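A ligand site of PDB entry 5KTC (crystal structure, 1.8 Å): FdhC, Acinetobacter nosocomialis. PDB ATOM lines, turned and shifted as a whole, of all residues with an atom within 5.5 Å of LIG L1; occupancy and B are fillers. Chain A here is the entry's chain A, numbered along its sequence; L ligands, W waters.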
ATOM      1  N   ILE A  24     -19.052   5.618   1.897  1.00  0.00           N
ATOM      2  CA  ILE A  24     -18.249   5.974   3.054  1.00  0.00           C
ATOM      3  C   ILE A  24     -18.825   5.344   4.316  1.00  0.00           C
ATOM      4  O   ILE A  24     -18.062   4.714   5.056  1.00  0.00           O
ATOM      5  CB  ILE A  24     -18.022   7.468   3.201  1.00  0.00           C
ATOM      6  CG1 ILE A  24     -17.147   7.975   2.042  1.00  0.00           C
ATOM      7  CG2 ILE A  24     -17.207   7.724   4.465  1.00  0.00           C
ATOM      8  CD1 ILE A  24     -16.933   9.465   1.995  1.00  0.00           C
ATOM      9  N   ARG A  28     -16.619   2.584   6.468  1.00  0.00           N
ATOM     10  CA  ARG A  28     -16.175   2.945   7.829  1.00  0.00           C
ATOM     11  C   ARG A  28     -16.846   2.085   8.931  1.00  0.00           C
ATOM     12  O   ARG A  28     -16.282   1.924  10.012  1.00  0.00           O
ATOM     13  CB  ARG A  28     -16.453   4.406   8.058  1.00  0.00           C
ATOM     14  CG  ARG A  28     -15.473   5.317   7.311  1.00  0.00           C
ATOM     15  CD  ARG A  28     -15.687   6.768   7.712  1.00  0.00           C
ATOM     16  NE  ARG A  28     -15.178   6.991   9.075  1.00  0.00           N
ATOM     17  CZ  ARG A  28     -13.949   7.382   9.400  1.00  0.00           C
ATOM     18  NH1 ARG A  28     -13.010   7.659   8.475  1.00  0.00           N
ATOM     19  NH2 ARG A  28     -13.624   7.438  10.704  1.00  0.00           N
ATOM     20  N   TYR A  36      -8.878   0.255  13.716  1.00  0.00           N
ATOM     21  CA  TYR A  36      -7.944   1.300  14.159  1.00  0.00           C
ATOM     22  C   TYR A  36      -8.286   2.714  13.615  1.00  0.00           C
ATOM     23  O   TYR A  36      -7.391   3.598  13.492  1.00  0.00           O
ATOM     24  CB  TYR A  36      -6.568   0.879  13.726  1.00  0.00           C
ATOM     25  CG  TYR A  36      -6.113  -0.451  14.275  1.00  0.00           C
ATOM     26  CD1 TYR A  36      -5.813  -0.605  15.631  1.00  0.00           C
ATOM     27  CD2 TYR A  36      -5.944  -1.522  13.444  1.00  0.00           C
ATOM     28  CE1 TYR A  36      -5.386  -1.826  16.121  1.00  0.00           C
ATOM     29  CE2 TYR A  36      -5.498  -2.717  13.912  1.00  0.00           C
ATOM     30  CZ  TYR A  36      -5.232  -2.883  15.258  1.00  0.00           C
ATOM     31  OH  TYR A  36      -4.764  -4.132  15.700  1.00  0.00           O
ATOM     32  N   ILE A  37      -9.547   2.917  13.266  1.00  0.00           N
ATOM     33  CA  ILE A  37      -9.984   4.224  12.850  1.00  0.00           C
ATOM     34  C   ILE A  37     -11.068   4.695  13.780  1.00  0.00           C
ATOM     35  O   ILE A  37     -11.551   3.900  14.608  1.00  0.00           O
ATOM     36  CB  ILE A  37     -10.395   4.266  11.352  1.00  0.00           C
ATOM     37  CG1 ILE A  37     -11.745   3.616  11.165  1.00  0.00           C
ATOM     38  CG2 ILE A  37      -9.336   3.539  10.524  1.00  0.00           C
ATOM     39  CD1 ILE A  37     -12.306   3.693   9.771  1.00  0.00           C
ATOM     40  N   SER A  38     -11.446   5.971  13.649  1.00  0.00           N
ATOM     41  CA  SER A  38     -12.463   6.567  14.520  1.00  0.00           C
ATOM     42  C   SER A  38     -13.858   6.043  14.228  1.00  0.00           C
ATOM     43  O   SER A  38     -14.245   5.902  13.071  1.00  0.00           O
ATOM     44  CB  SER A  38     -12.504   8.092  14.411  1.00  0.00           C
ATOM     45  OG  SER A  38     -11.312   8.736  14.861  1.00  0.00           O
ATOM     46  N   LYS A  39     -14.652   5.739  15.269  1.00  0.00           N
ATOM     47  CA  LYS A  39     -16.090   5.475  15.068  1.00  0.00           C
ATOM     48  C   LYS A  39     -16.737   6.591  14.310  1.00  0.00           C
ATOM     49  O   LYS A  39     -16.482   7.753  14.554  1.00  0.00           O
ATOM     50  CB  LYS A  39     -16.849   5.473  16.409  1.00  0.00           C
ATOM     51  CG  LYS A  39     -16.407   4.452  17.384  1.00  0.00           C
ATOM     52  CD  LYS A  39     -17.268   4.518  18.643  1.00  0.00           C
ATOM     53  CE  LYS A  39     -16.946   3.296  19.469  1.00  0.00           C
ATOM     54  NZ  LYS A  39     -17.885   3.086  20.581  1.00  0.00           N
ATOM     55  N   SER A  40     -17.647   6.243  13.425  1.00  0.00           N
ATOM     56  CA  SER A  40     -18.437   7.254  12.754  1.00  0.00           C
ATOM     57  C   SER A  40     -19.812   6.738  12.382  1.00  0.00           C
ATOM     58  O   SER A  40     -20.027   5.524  12.327  1.00  0.00           O
ATOM     59  CB  SER A  40     -17.707   7.712  11.462  1.00  0.00           C
ATOM     60  OG  SER A  40     -17.608   6.654  10.512  1.00  0.00           O
ATOM     61  N   THR A  41     -20.700   7.688  12.070  1.00  0.00           N
ATOM     62  CA  THR A  41     -22.069   7.383  11.775  1.00  0.00           C
ATOM     63  C   THR A  41     -22.248   6.328  10.688  1.00  0.00           C
ATOM     64  O   THR A  41     -21.485   6.297   9.686  1.00  0.00           O
ATOM     65  CB  THR A  41     -22.850   8.655  11.385  1.00  0.00           C
ATOM     66  OG1 THR A  41     -24.237   8.300  11.284  1.00  0.00           O
ATOM     67  CG2 THR A  41     -22.409   9.254  10.002  1.00  0.00           C
ATOM     68  N   GLN A  47     -23.731  11.236   7.360  1.00  0.00           N
ATOM     69  CA  GLN A  47     -22.453  11.261   6.634  1.00  0.00           C
ATOM     70  C   GLN A  47     -22.476  12.336   5.508  1.00  0.00           C
ATOM     71  O   GLN A  47     -21.490  13.011   5.309  1.00  0.00           O
ATOM     72  CB  GLN A  47     -22.106   9.888   6.123  1.00  0.00           C
ATOM     73  CG  GLN A  47     -20.831   9.779   5.308  1.00  0.00           C
ATOM     74  CD  GLN A  47     -19.587  10.103   6.050  1.00  0.00           C
ATOM     75  OE1 GLN A  47     -19.394   9.686   7.161  1.00  0.00           O
ATOM     76  NE2 GLN A  47     -18.668  10.825   5.401  1.00  0.00           N
ATOM     77  N   TRP A  50     -21.684  15.519   7.211  1.00  0.00           N
ATOM     78  CA  TRP A  50     -20.223  15.562   7.458  1.00  0.00           C
ATOM     79  C   TRP A  50     -19.505  16.021   6.174  1.00  0.00           C
ATOM     80  O   TRP A  50     -18.588  16.855   6.227  1.00  0.00           O
ATOM     81  CB  TRP A  50     -19.685  14.178   7.909  1.00  0.00           C
ATOM     82  CG  TRP A  50     -18.304  14.242   8.556  1.00  0.00           C
ATOM     83  CD1 TRP A  50     -17.996  14.258   9.923  1.00  0.00           C
ATOM     84  CD2 TRP A  50     -17.059  14.317   7.879  1.00  0.00           C
ATOM     85  NE1 TRP A  50     -16.630  14.357  10.097  1.00  0.00           N
ATOM     86  CE2 TRP A  50     -16.035  14.417   8.875  1.00  0.00           C
ATOM     87  CE3 TRP A  50     -16.680  14.350   6.520  1.00  0.00           C
ATOM     88  CZ2 TRP A  50     -14.676  14.528   8.538  1.00  0.00           C
ATOM     89  CZ3 TRP A  50     -15.298  14.470   6.215  1.00  0.00           C
ATOM     90  CH2 TRP A  50     -14.342  14.549   7.216  1.00  0.00           C
ATOM     91  N   TYR A  65     -10.263  15.515   0.554  1.00  0.00           N
ATOM     92  CA  TYR A  65     -10.723  14.162   0.902  1.00  0.00           C
ATOM     93  C   TYR A  65     -11.087  13.468  -0.388  1.00  0.00           C
ATOM     94  O   TYR A  65     -11.786  14.069  -1.194  1.00  0.00           O
ATOM     95  CB  TYR A  65     -11.965  14.303   1.748  1.00  0.00           C
ATOM     96  CG  TYR A  65     -12.534  13.124   2.438  1.00  0.00           C
ATOM     97  CD1 TYR A  65     -11.867  11.925   2.562  1.00  0.00           C
ATOM     98  CD2 TYR A  65     -13.793  13.225   3.026  1.00  0.00           C
ATOM     99  CE1 TYR A  65     -12.428  10.859   3.267  1.00  0.00           C
ATOM    100  CE2 TYR A  65     -14.366  12.163   3.726  1.00  0.00           C
ATOM    101  CZ  TYR A  65     -13.684  10.980   3.846  1.00  0.00           C
ATOM    102  OH  TYR A  65     -14.259   9.875   4.546  1.00  0.00           O
ATOM    103  N   ARG A  81      -7.402  10.998   3.018  1.00  0.00           N
ATOM    104  CA  ARG A  81      -7.609  12.466   3.320  1.00  0.00           C
ATOM    105  C   ARG A  81      -6.349  13.178   3.713  1.00  0.00           C
ATOM    106  O   ARG A  81      -5.542  12.640   4.458  1.00  0.00           O
ATOM    107  CB  ARG A  81      -8.623  12.571   4.452  1.00  0.00           C
ATOM    108  CG  ARG A  81      -9.215  13.939   4.739  1.00  0.00           C
ATOM    109  CD  ARG A  81     -10.510  13.836   5.589  1.00  0.00           C
ATOM    110  NE  ARG A  81     -10.225  13.262   6.880  1.00  0.00           N
ATOM    111  CZ  ARG A  81     -10.227  13.807   8.115  1.00  0.00           C
ATOM    112  NH1 ARG A  81     -10.616  15.050   8.399  1.00  0.00           N
ATOM    113  NH2 ARG A  81      -9.858  13.031   9.116  1.00  0.00           N
ATOM    114  N   TYR A  83      -5.434  16.806   5.624  1.00  0.00           N
ATOM    115  CA  TYR A  83      -6.176  17.655   6.576  1.00  0.00           C
ATOM    116  C   TYR A  83      -5.182  18.278   7.592  1.00  0.00           C
ATOM    117  O   TYR A  83      -3.994  17.896   7.700  1.00  0.00           O
ATOM    118  CB  TYR A  83      -7.327  16.800   7.219  1.00  0.00           C
ATOM    119  CG  TYR A  83      -6.882  15.680   8.167  1.00  0.00           C
ATOM    120  CD1 TYR A  83      -6.344  14.507   7.688  1.00  0.00           C
ATOM    121  CD2 TYR A  83      -7.017  15.795   9.596  1.00  0.00           C
ATOM    122  CE1 TYR A  83      -5.959  13.494   8.550  1.00  0.00           C
ATOM    123  CE2 TYR A  83      -6.660  14.781  10.467  1.00  0.00           C
ATOM    124  CZ  TYR A  83      -6.101  13.624   9.955  1.00  0.00           C
ATOM    125  OH  TYR A  83      -5.753  12.555  10.770  1.00  0.00           O
ATOM    126  N   TRP A  94      -2.203  13.448   7.001  1.00  0.00           N
ATOM    127  CA  TRP A  94      -3.016  12.578   6.175  1.00  0.00           C
ATOM    128  C   TRP A  94      -3.425  11.338   6.954  1.00  0.00           C
ATOM    129  O   TRP A  94      -2.862  10.991   8.010  1.00  0.00           O
ATOM    130  CB  TRP A  94      -2.351  12.225   4.848  1.00  0.00           C
ATOM    131  CG  TRP A  94      -1.254  11.204   4.816  1.00  0.00           C
ATOM    132  CD1 TRP A  94       0.052  11.386   5.141  1.00  0.00           C
ATOM    133  CD2 TRP A  94      -1.378   9.849   4.335  1.00  0.00           C
ATOM    134  NE1 TRP A  94       0.750  10.204   4.902  1.00  0.00           N
ATOM    135  CE2 TRP A  94      -0.099   9.272   4.364  1.00  0.00           C
ATOM    136  CE3 TRP A  94      -2.450   9.087   3.853  1.00  0.00           C
ATOM    137  CZ2 TRP A  94       0.142   7.951   3.945  1.00  0.00           C
ATOM    138  CZ3 TRP A  94      -2.204   7.768   3.404  1.00  0.00           C
ATOM    139  CH2 TRP A  94      -0.927   7.219   3.465  1.00  0.00           C
ATOM    140  N   GLY A  95      -4.436  10.718   6.425  1.00  0.00           N
ATOM    141  CA  GLY A  95      -5.075   9.599   7.088  1.00  0.00           C
ATOM    142  C   GLY A  95      -6.433   9.328   6.519  1.00  0.00           C
ATOM    143  O   GLY A  95      -6.636   9.422   5.287  1.00  0.00           O
ATOM    144  N   SER A  96      -7.386   8.979   7.385  1.00  0.00           N
ATOM    145  CA  SER A  96      -8.646   8.386   6.934  1.00  0.00           C
ATOM    146  C   SER A  96      -8.443   7.333   5.816  1.00  0.00           C
ATOM    147  O   SER A  96      -9.195   7.296   4.815  1.00  0.00           O
ATOM    148  CB  SER A  96      -9.691   9.427   6.537  1.00  0.00           C
ATOM    149  OG  SER A  96      -9.896  10.441   7.501  1.00  0.00           O
ATOM    150  N   TRP A  97      -7.428   6.521   5.993  1.00  0.00           N
ATOM    151  CA  TRP A  97      -6.847   5.774   4.876  1.00  0.00           C
ATOM    152  C   TRP A  97      -7.398   4.374   4.998  1.00  0.00           C
ATOM    153  O   TRP A  97      -7.033   3.616   5.946  1.00  0.00           O
ATOM    154  CB  TRP A  97      -5.365   5.730   5.002  1.00  0.00           C
ATOM    155  CG  TRP A  97      -4.636   5.120   3.839  1.00  0.00           C
ATOM    156  CD1 TRP A  97      -4.977   5.168   2.519  1.00  0.00           C
ATOM    157  CD2 TRP A  97      -3.396   4.419   3.919  1.00  0.00           C
ATOM    158  NE1 TRP A  97      -3.992   4.522   1.775  1.00  0.00           N
ATOM    159  CE2 TRP A  97      -3.010   4.077   2.607  1.00  0.00           C
ATOM    160  CE3 TRP A  97      -2.568   4.036   4.992  1.00  0.00           C
ATOM    161  CZ2 TRP A  97      -1.875   3.358   2.322  1.00  0.00           C
ATOM    162  CZ3 TRP A  97      -1.397   3.315   4.718  1.00  0.00           C
ATOM    163  CH2 TRP A  97      -1.056   3.005   3.368  1.00  0.00           C
ATOM    164  N   PHE A 130       1.465  12.212  10.529  1.00  0.00           N
ATOM    165  CA  PHE A 130       0.315  11.305  10.736  1.00  0.00           C
ATOM    166  C   PHE A 130       0.593  10.376  11.923  1.00  0.00           C
ATOM    167  O   PHE A 130       1.703  10.308  12.440  1.00  0.00           O
ATOM    168  CB  PHE A 130       0.017  10.464   9.474  1.00  0.00           C
ATOM    169  CG  PHE A 130       1.202   9.701   8.984  1.00  0.00           C
ATOM    170  CD1 PHE A 130       2.092  10.288   8.113  1.00  0.00           C
ATOM    171  CD2 PHE A 130       1.462   8.385   9.447  1.00  0.00           C
ATOM    172  CE1 PHE A 130       3.209   9.567   7.649  1.00  0.00           C
ATOM    173  CE2 PHE A 130       2.585   7.675   9.001  1.00  0.00           C
ATOM    174  CZ  PHE A 130       3.444   8.275   8.099  1.00  0.00           C
ATOM    175  N   GLU A 131      -0.444   9.644  12.331  1.00  0.00           N
ATOM    176  CA  GLU A 131      -0.317   8.679  13.412  1.00  0.00           C
ATOM    177  C   GLU A 131      -0.972   7.346  13.055  1.00  0.00           C
ATOM    178  O   GLU A 131      -1.839   7.294  12.184  1.00  0.00           O
ATOM    179  CB  GLU A 131      -0.951   9.238  14.671  1.00  0.00           C
ATOM    180  CG  GLU A 131      -2.408   9.554  14.656  1.00  0.00           C
ATOM    181  CD  GLU A 131      -2.782  10.985  14.389  1.00  0.00           C
ATOM    182  OE1 GLU A 131      -3.867  11.224  13.846  1.00  0.00           O
ATOM    183  OE2 GLU A 131      -2.007  11.890  14.721  1.00  0.00           O
ATOM    184  N   VAL A 132      -0.558   6.282  13.756  1.00  0.00           N
ATOM    185  CA  VAL A 132      -1.022   4.933  13.516  1.00  0.00           C
ATOM    186  C   VAL A 132      -1.192   4.277  14.877  1.00  0.00           C
ATOM    187  O   VAL A 132      -0.308   4.401  15.741  1.00  0.00           O
ATOM    188  CB  VAL A 132       0.034   4.147  12.758  1.00  0.00           C
ATOM    189  CG1 VAL A 132      -0.395   2.717  12.489  1.00  0.00           C
ATOM    190  CG2 VAL A 132       0.403   4.863  11.449  1.00  0.00           C
ATOM    191  N   MET A 133      -2.326   3.648  15.123  1.00  0.00           N
ATOM    192  CA  MET A 133      -2.540   3.014  16.434  1.00  0.00           C
ATOM    193  C   MET A 133      -1.570   1.922  16.723  1.00  0.00           C
ATOM    194  O   MET A 133      -1.254   1.139  15.881  1.00  0.00           O
ATOM    195  CB  MET A 133      -3.965   2.483  16.591  1.00  0.00           C
ATOM    196  CG  MET A 133      -4.978   3.590  16.908  1.00  0.00           C
ATOM    197  SD  MET A 133      -6.582   2.936  17.438  1.00  0.00           S
ATOM    198  CE  MET A 133      -6.263   2.473  19.159  1.00  0.00           C
ATOM    199  N   VAL A 139       0.723  -1.594   9.349  1.00  0.00           N
ATOM    200  CA  VAL A 139       0.669  -0.178   8.884  1.00  0.00           C
ATOM    201  C   VAL A 139       1.917   0.568   9.379  1.00  0.00           C
ATOM    202  O   VAL A 139       2.515   1.343   8.649  1.00  0.00           O
ATOM    203  CB  VAL A 139      -0.675   0.464   9.322  1.00  0.00           C
ATOM    204  CG1 VAL A 139      -0.763   1.953   8.913  1.00  0.00           C
ATOM    205  CG2 VAL A 139      -1.806  -0.338   8.703  1.00  0.00           C
ATOM    206  N   HIS A 143       4.665   2.231   6.630  1.00  0.00           N
ATOM    207  CA  HIS A 143       5.197   3.600   6.722  1.00  0.00           C
ATOM    208  C   HIS A 143       6.722   3.643   6.972  1.00  0.00           C
ATOM    209  O   HIS A 143       7.434   4.403   6.289  1.00  0.00           O
ATOM    210  CB  HIS A 143       4.473   4.432   7.795  1.00  0.00           C
ATOM    211  CG  HIS A 143       3.038   4.708   7.466  1.00  0.00           C
ATOM    212  ND1 HIS A 143       2.659   5.353   6.317  1.00  0.00           N
ATOM    213  CD2 HIS A 143       1.899   4.415   8.124  1.00  0.00           C
ATOM    214  CE1 HIS A 143       1.347   5.479   6.297  1.00  0.00           C
ATOM    215  NE2 HIS A 143       0.858   4.910   7.387  1.00  0.00           N
ATOM    216  N   ASN A 157      -1.080   5.657  20.170  1.00  0.00           N
ATOM    217  CA  ASN A 157      -0.465   5.892  18.833  1.00  0.00           C
ATOM    218  C   ASN A 157       1.030   5.962  18.802  1.00  0.00           C
ATOM    219  O   ASN A 157       1.704   6.218  19.814  1.00  0.00           O
ATOM    220  CB  ASN A 157      -0.907   7.283  18.333  1.00  0.00           C
ATOM    221  CG  ASN A 157      -2.393   7.398  18.126  1.00  0.00           C
ATOM    222  OD1 ASN A 157      -3.019   6.433  17.749  1.00  0.00           O
ATOM    223  ND2 ASN A 157      -2.976   8.584  18.366  1.00  0.00           N
HETATM  224  O1  LIG L   1      -5.203   6.918   8.592  1.00  0.00           O
HETATM  225  C1  LIG L   1      -4.365   7.321   9.388  1.00  0.00           C
HETATM  226  C2  LIG L   1      -2.938   7.557   9.029  1.00  0.00           C
HETATM  227  C3  LIG L   1      -2.511   6.750   7.827  1.00  0.00           C
HETATM  228  O2  LIG L   1      -1.978   5.468   8.216  1.00  0.00           O
HETATM  229  C4  LIG L   1      -1.408   7.463   7.081  1.00  0.00           C
HETATM  230  N1  LIG L   1      -4.700   7.619  10.712  1.00  0.00           N
HETATM  231  C5  LIG L   1      -6.103   7.753  11.103  1.00  0.00           C
HETATM  232  C6  LIG L   1      -6.388   7.021  12.432  1.00  0.00           C
HETATM  233  O3  LIG L   1      -5.525   7.519  13.362  1.00  0.00           O
HETATM  234  C7  LIG L   1      -7.769   7.292  12.987  1.00  0.00           C
HETATM  235  C8  LIG L   1      -7.974   6.804  14.443  1.00  0.00           C
HETATM  236  O4  LIG L   1      -8.043   8.692  12.987  1.00  0.00           O
HETATM  237  C9  LIG L   1      -6.443   9.229  11.260  1.00  0.00           C
HETATM  238  O5  LIG L   1      -6.400   9.924  10.010  1.00  0.00           O
HETATM  239  C10 LIG L   1      -7.831   9.369  11.742  1.00  0.00           C
HETATM  240  O6  LIG L   1      -8.681   8.828  10.736  1.00  0.00           O
HETATM  241  P1  LIG L   1     -10.234   9.061  10.752  1.00  0.00           P
HETATM  242  O7  LIG L   1     -10.945   8.129  11.661  1.00  0.00           O
HETATM  243  O8  LIG L   1     -10.641   8.828   9.290  1.00  0.00           O
HETATM  244  O9  LIG L   1     -10.585  10.604  10.924  1.00  0.00           O
HETATM  245  P2  LIG L   1     -10.724  11.532  12.222  1.00  0.00           P
HETATM  246  O10 LIG L   1      -9.892  12.736  11.993  1.00  0.00           O
HETATM  247  O11 LIG L   1     -10.290  10.684  13.411  1.00  0.00           O
HETATM  248  O12 LIG L   1     -12.262  11.827  12.145  1.00  0.00           O
HETATM  249  C11 LIG L   1     -12.807  12.993  12.772  1.00  0.00           C
HETATM  250  C12 LIG L   1     -14.234  12.704  13.158  1.00  0.00           C
HETATM  251  C13 LIG L   1     -14.431  11.338  13.851  1.00  0.00           C
HETATM  252  O13 LIG L   1     -15.468  11.392  14.849  1.00  0.00           O
HETATM  253  C14 LIG L   1     -14.947  10.416  12.764  1.00  0.00           C
HETATM  254  C15 LIG L   1     -15.705  11.382  11.889  1.00  0.00           C
HETATM  255  O14 LIG L   1     -15.050  12.677  11.986  1.00  0.00           O
HETATM  256  N2  LIG L   1     -15.703  11.118  10.434  1.00  0.00           N
HETATM  257  C16 LIG L   1     -14.551  11.183   9.714  1.00  0.00           C
HETATM  258  C17 LIG L   1     -14.582  10.988   8.330  1.00  0.00           C
HETATM  259  C18 LIG L   1     -13.343  11.070   7.476  1.00  0.00           C
HETATM  260  C19 LIG L   1     -15.852  10.692   7.740  1.00  0.00           C
HETATM  261  O15 LIG L   1     -15.931  10.556   6.452  1.00  0.00           O
HETATM  262  N3  LIG L   1     -16.969  10.636   8.482  1.00  0.00           N
HETATM  263  C20 LIG L   1     -16.887  10.878   9.790  1.00  0.00           C
HETATM  264  O16 LIG L   1     -17.991  10.798  10.516  1.00  0.00           O
HETATM  265  N1  LG2 L   2       7.347  -1.468  -1.563  1.00  0.00           N
HETATM  266  C1  LG2 L   2       6.860  -2.505  -2.295  1.00  0.00           C
HETATM  267  N2  LG2 L   2       5.750  -3.168  -1.942  1.00  0.00           N
HETATM  268  C2  LG2 L   2       5.058  -2.744  -0.896  1.00  0.00           C
HETATM  269  C3  LG2 L   2       5.514  -1.600  -0.082  1.00  0.00           C
HETATM  270  C4  LG2 L   2       6.746  -0.963  -0.481  1.00  0.00           C
HETATM  271  N3  LG2 L   2       7.242   0.077   0.191  1.00  0.00           N
HETATM  272  N4  LG2 L   2       4.626  -1.414   0.883  1.00  0.00           N
HETATM  273  C5  LG2 L   2       3.682  -2.373   0.730  1.00  0.00           C
HETATM  274  N5  LG2 L   2       3.951  -3.168  -0.329  1.00  0.00           N
HETATM  275  C6  LG2 L   2       3.144  -4.299  -0.833  1.00  0.00           C
HETATM  276  C7  LG2 L   2       2.680  -5.159   0.345  1.00  0.00           C
HETATM  277  O1  LG2 L   2       3.644  -6.153   0.727  1.00  0.00           O
HETATM  278  C8  LG2 L   2       1.384  -5.708  -0.155  1.00  0.00           C
HETATM  279  O2  LG2 L   2       1.688  -6.767  -1.066  1.00  0.00           O
HETATM  280  P1  LG2 L   2       1.421  -8.296  -0.648  1.00  0.00           P
HETATM  281  O3  LG2 L   2       0.058  -8.550  -1.307  1.00  0.00           O
HETATM  282  O4  LG2 L   2       2.613  -8.808  -1.405  1.00  0.00           O
HETATM  283  O5  LG2 L   2       1.440  -8.368   0.858  1.00  0.00           O
HETATM  284  C9  LG2 L   2       0.808  -4.555  -0.950  1.00  0.00           C
HETATM  285  O6  LG2 L   2       1.934  -3.800  -1.430  1.00  0.00           O
HETATM  286  C10 LG2 L   2      -0.209  -3.741  -0.178  1.00  0.00           C
HETATM  287  O7  LG2 L   2       0.366  -3.235   1.006  1.00  0.00           O
HETATM  288  P2  LG2 L   2      -0.252  -3.609   2.408  1.00  0.00           P
HETATM  289  O8  LG2 L   2       0.706  -3.138   3.480  1.00  0.00           O
HETATM  290  O9  LG2 L   2      -0.895  -4.971   2.474  1.00  0.00           O
HETATM  291  O10 LG2 L   2      -1.481  -2.585   2.629  1.00  0.00           O
HETATM  292  P3  LG2 L   2      -3.029  -2.785   2.658  1.00  0.00           P
HETATM  293  O11 LG2 L   2      -3.609  -3.278   1.359  1.00  0.00           O
HETATM  294  O12 LG2 L   2      -3.471  -3.551   3.895  1.00  0.00           O
HETATM  295  O13 LG2 L   2      -3.556  -1.292   2.810  1.00  0.00           O
HETATM  296  C11 LG2 L   2      -4.548   0.021   4.605  1.00  0.00           C
HETATM  297  C12 LG2 L   2      -3.271  -0.593   4.017  1.00  0.00           C
HETATM  298  C13 LG2 L   2      -4.169   0.683   5.906  1.00  0.00           C
HETATM  299  C14 LG2 L   2      -5.137   1.059   3.646  1.00  0.00           C
HETATM  300  C15 LG2 L   2      -5.585  -1.101   4.837  1.00  0.00           C
HETATM  301  O14 LG2 L   2      -4.863  -2.185   5.504  1.00  0.00           O
HETATM  302  C16 LG2 L   2      -6.793  -0.681   5.580  1.00  0.00           C
HETATM  303  O15 LG2 L   2      -7.791  -0.109   5.098  1.00  0.00           O
HETATM  304  N6  LG2 L   2      -6.733  -0.952   6.905  1.00  0.00           N
HETATM  305  C17 LG2 L   2      -7.791  -0.596   7.758  1.00  0.00           C
HETATM  306  C18 LG2 L   2      -7.971   0.882   8.024  1.00  0.00           C
HETATM  307  C19 LG2 L   2      -6.754   1.420   8.728  1.00  0.00           C
HETATM  308  O16 LG2 L   2      -6.333   0.825   9.742  1.00  0.00           O
HETATM  309  N7  LG2 L   2      -6.180   2.472   8.197  1.00  0.00           N
HETATM  310  C20 LG2 L   2      -4.918   3.013   8.712  1.00  0.00           C
HETATM  311  C21 LG2 L   2      -5.103   3.815  10.015  1.00  0.00           C
HETATM  312  S1  LG2 L   2      -3.449   4.200  10.714  1.00  0.00           S
HETATM  313  O   HOH W   1     -19.714  10.325  12.407  1.00  0.00           O
HETATM  314  O   HOH W   2      -7.249  12.795  12.883  1.00  0.00           O
HETATM  315  O   HOH W   3     -10.745  15.421  11.138  1.00  0.00           O
HETATM  316  O   HOH W   4      -5.762   9.583  15.201  1.00  0.00           O
HETATM  317  O   HOH W   5      -3.003  10.523  11.016  1.00  0.00           O
HETATM  318  O   HOH W   6     -15.661   8.843  16.685  1.00  0.00           O
HETATM  319  O   HOH W   7      -7.904  11.081  14.812  1.00  0.00           O
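Water W1 lies within hydrogen-bond range of an oxygen (O16) of LIG L1 (2.6 Å) and the backbone NH (N) of Thr 41 (2.8 Å).
Water W4 lies within hydrogen-bond range of O3 of LIG L1 (2.8 Å) and OE1 of Glu 131 (2.8 Å).
Water W2 bridges OH of Tyr 83 (2.6 Å) and O10 of LIG L1 (2.8 Å).
Water W3 lies within hydrogen-bond range of NH1 of Arg 81 (2.8 Å) and O10 of LIG L1 (2.9 Å).
Water W6 bridges O of Lys 39 (2.5 Å) and O13 of LIG L1 (3.1 Å).
Water W5 lies within hydrogen-bond range of the backbone NH (N) of Glu 131 (3.0 Å), the backbone carbonyl oxygen (O) of Trp 94 (3.0 Å), a nitrogen (N1) of LIG L1 (3.4 Å) and the side-chain hydroxyl (OH) of Tyr 83 (3.4 Å).
N of Ser 96 sits at hydrogen-bond distance from O5 of LIG L1, 3.0 Å away.
An oxygen (O8) of LIG L1 sits at hydrogen-bond distance from the side-chain hydroxyl (OG) of Ser 96 (2.5 Å).
The side-chain hydroxyl of Tyr 65 lies within hydrogen-bond range of an oxygen (O15) of LIG L1 (2.6 Å).
An oxygen (O7) of LIG L1 sits at hydrogen-bond distance from the backbone NH (N) of Ser 38 (3.0 Å).
The side-chain hydroxyl (OG) of Ser 38 is in hydrogen-bond range of an oxygen (O11) of LIG L1 (2.6 Å).
O8 of LIG L1 lies within salt-bridge range of NH1 of Arg 28 (2.8 Å).
O5 of LIG L1 is in hydrogen-bond range of OH of Tyr 83 (2.8 Å).
NH2 of Arg 81 lies within salt-bridge range of O10 of LIG L1, at 2.9 Å.
N3 of LIG L1 sits at hydrogen-bond distance from OE1 of Gln 47, 2.9 Å away.
An oxygen (O14) of LIG L1 lies within hydrogen-bond range of the indole nitrogen of Trp 50 (3.0 Å).
A ring nitrogen (NE2) of His 143 lies within hydrogen-bond range of an oxygen (O2) of LIG L1.
A nitrogen (N1) of LIG L1 sits at hydrogen-bond distance from the backbone carbonyl oxygen (O) of Glu 131 (3.2 Å).
The backbone NH (N) of Trp 97 lies within hydrogen-bond range of an oxygen (O1) of LIG L1, 3.4 Å away.
S1 of LG2 L2 sits close to O of Glu 131 (3.8 Å).
O of Trp 97 lies within hydrogen-bond range of N7 of LG2 L2 (2.7 Å).
S1 of LG2 L2 lies close to O2 of LIG L1, at 3.2 Å.
Merely in contact with LIG L1: Gly 95, Ser 40, Tyr 36, Trp 94, Lys 39, Ile 37, Ile 24, Val 139 and Phe 130.
Hydrophobic or aromatic side chains within 4 Å of LIG L1: Ile 24, Ile 37, Trp 50, Tyr 65, Tyr 83, Trp 94, Trp 97, Phe 130, Val 139 and His 143.
20 residues have an atom within 4 Å of LIG L1: Ile 24, Arg 28, Tyr 36, Ile 37, Ser 38, Lys 39, Ser 40, Gln 47, Trp 50, Tyr 65, Arg 81, Tyr 83, Trp 94, Gly 95, Ser 96, Trp 97, Phe 130, Glu 131, Val 139 and His 143.
Along chain A the residues within 4 Å of LIG L1 span positions 24 to 143.
The nearest printed residue that does not touch LIG L1 is Val 132 (4.1 Å).
The side-chain hydroxyl (OG) of Ser 96 lies within hydrogen-bond range of the guanidinium group (NE) of Arg 81, at 2.9 Å.
The backbone carbonyl oxygen (O) of Ser 38 is in hydrogen-bond range of the guanidinium group (NH2) of Arg 28, at 2.9 Å.
NE of Arg 28 is in hydrogen-bond range of OG of Ser 40 (2.8 Å).
The backbone carbonyl oxygen (O) of Gly 95 lies within hydrogen-bond range of the backbone NH (N) of Arg 81.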
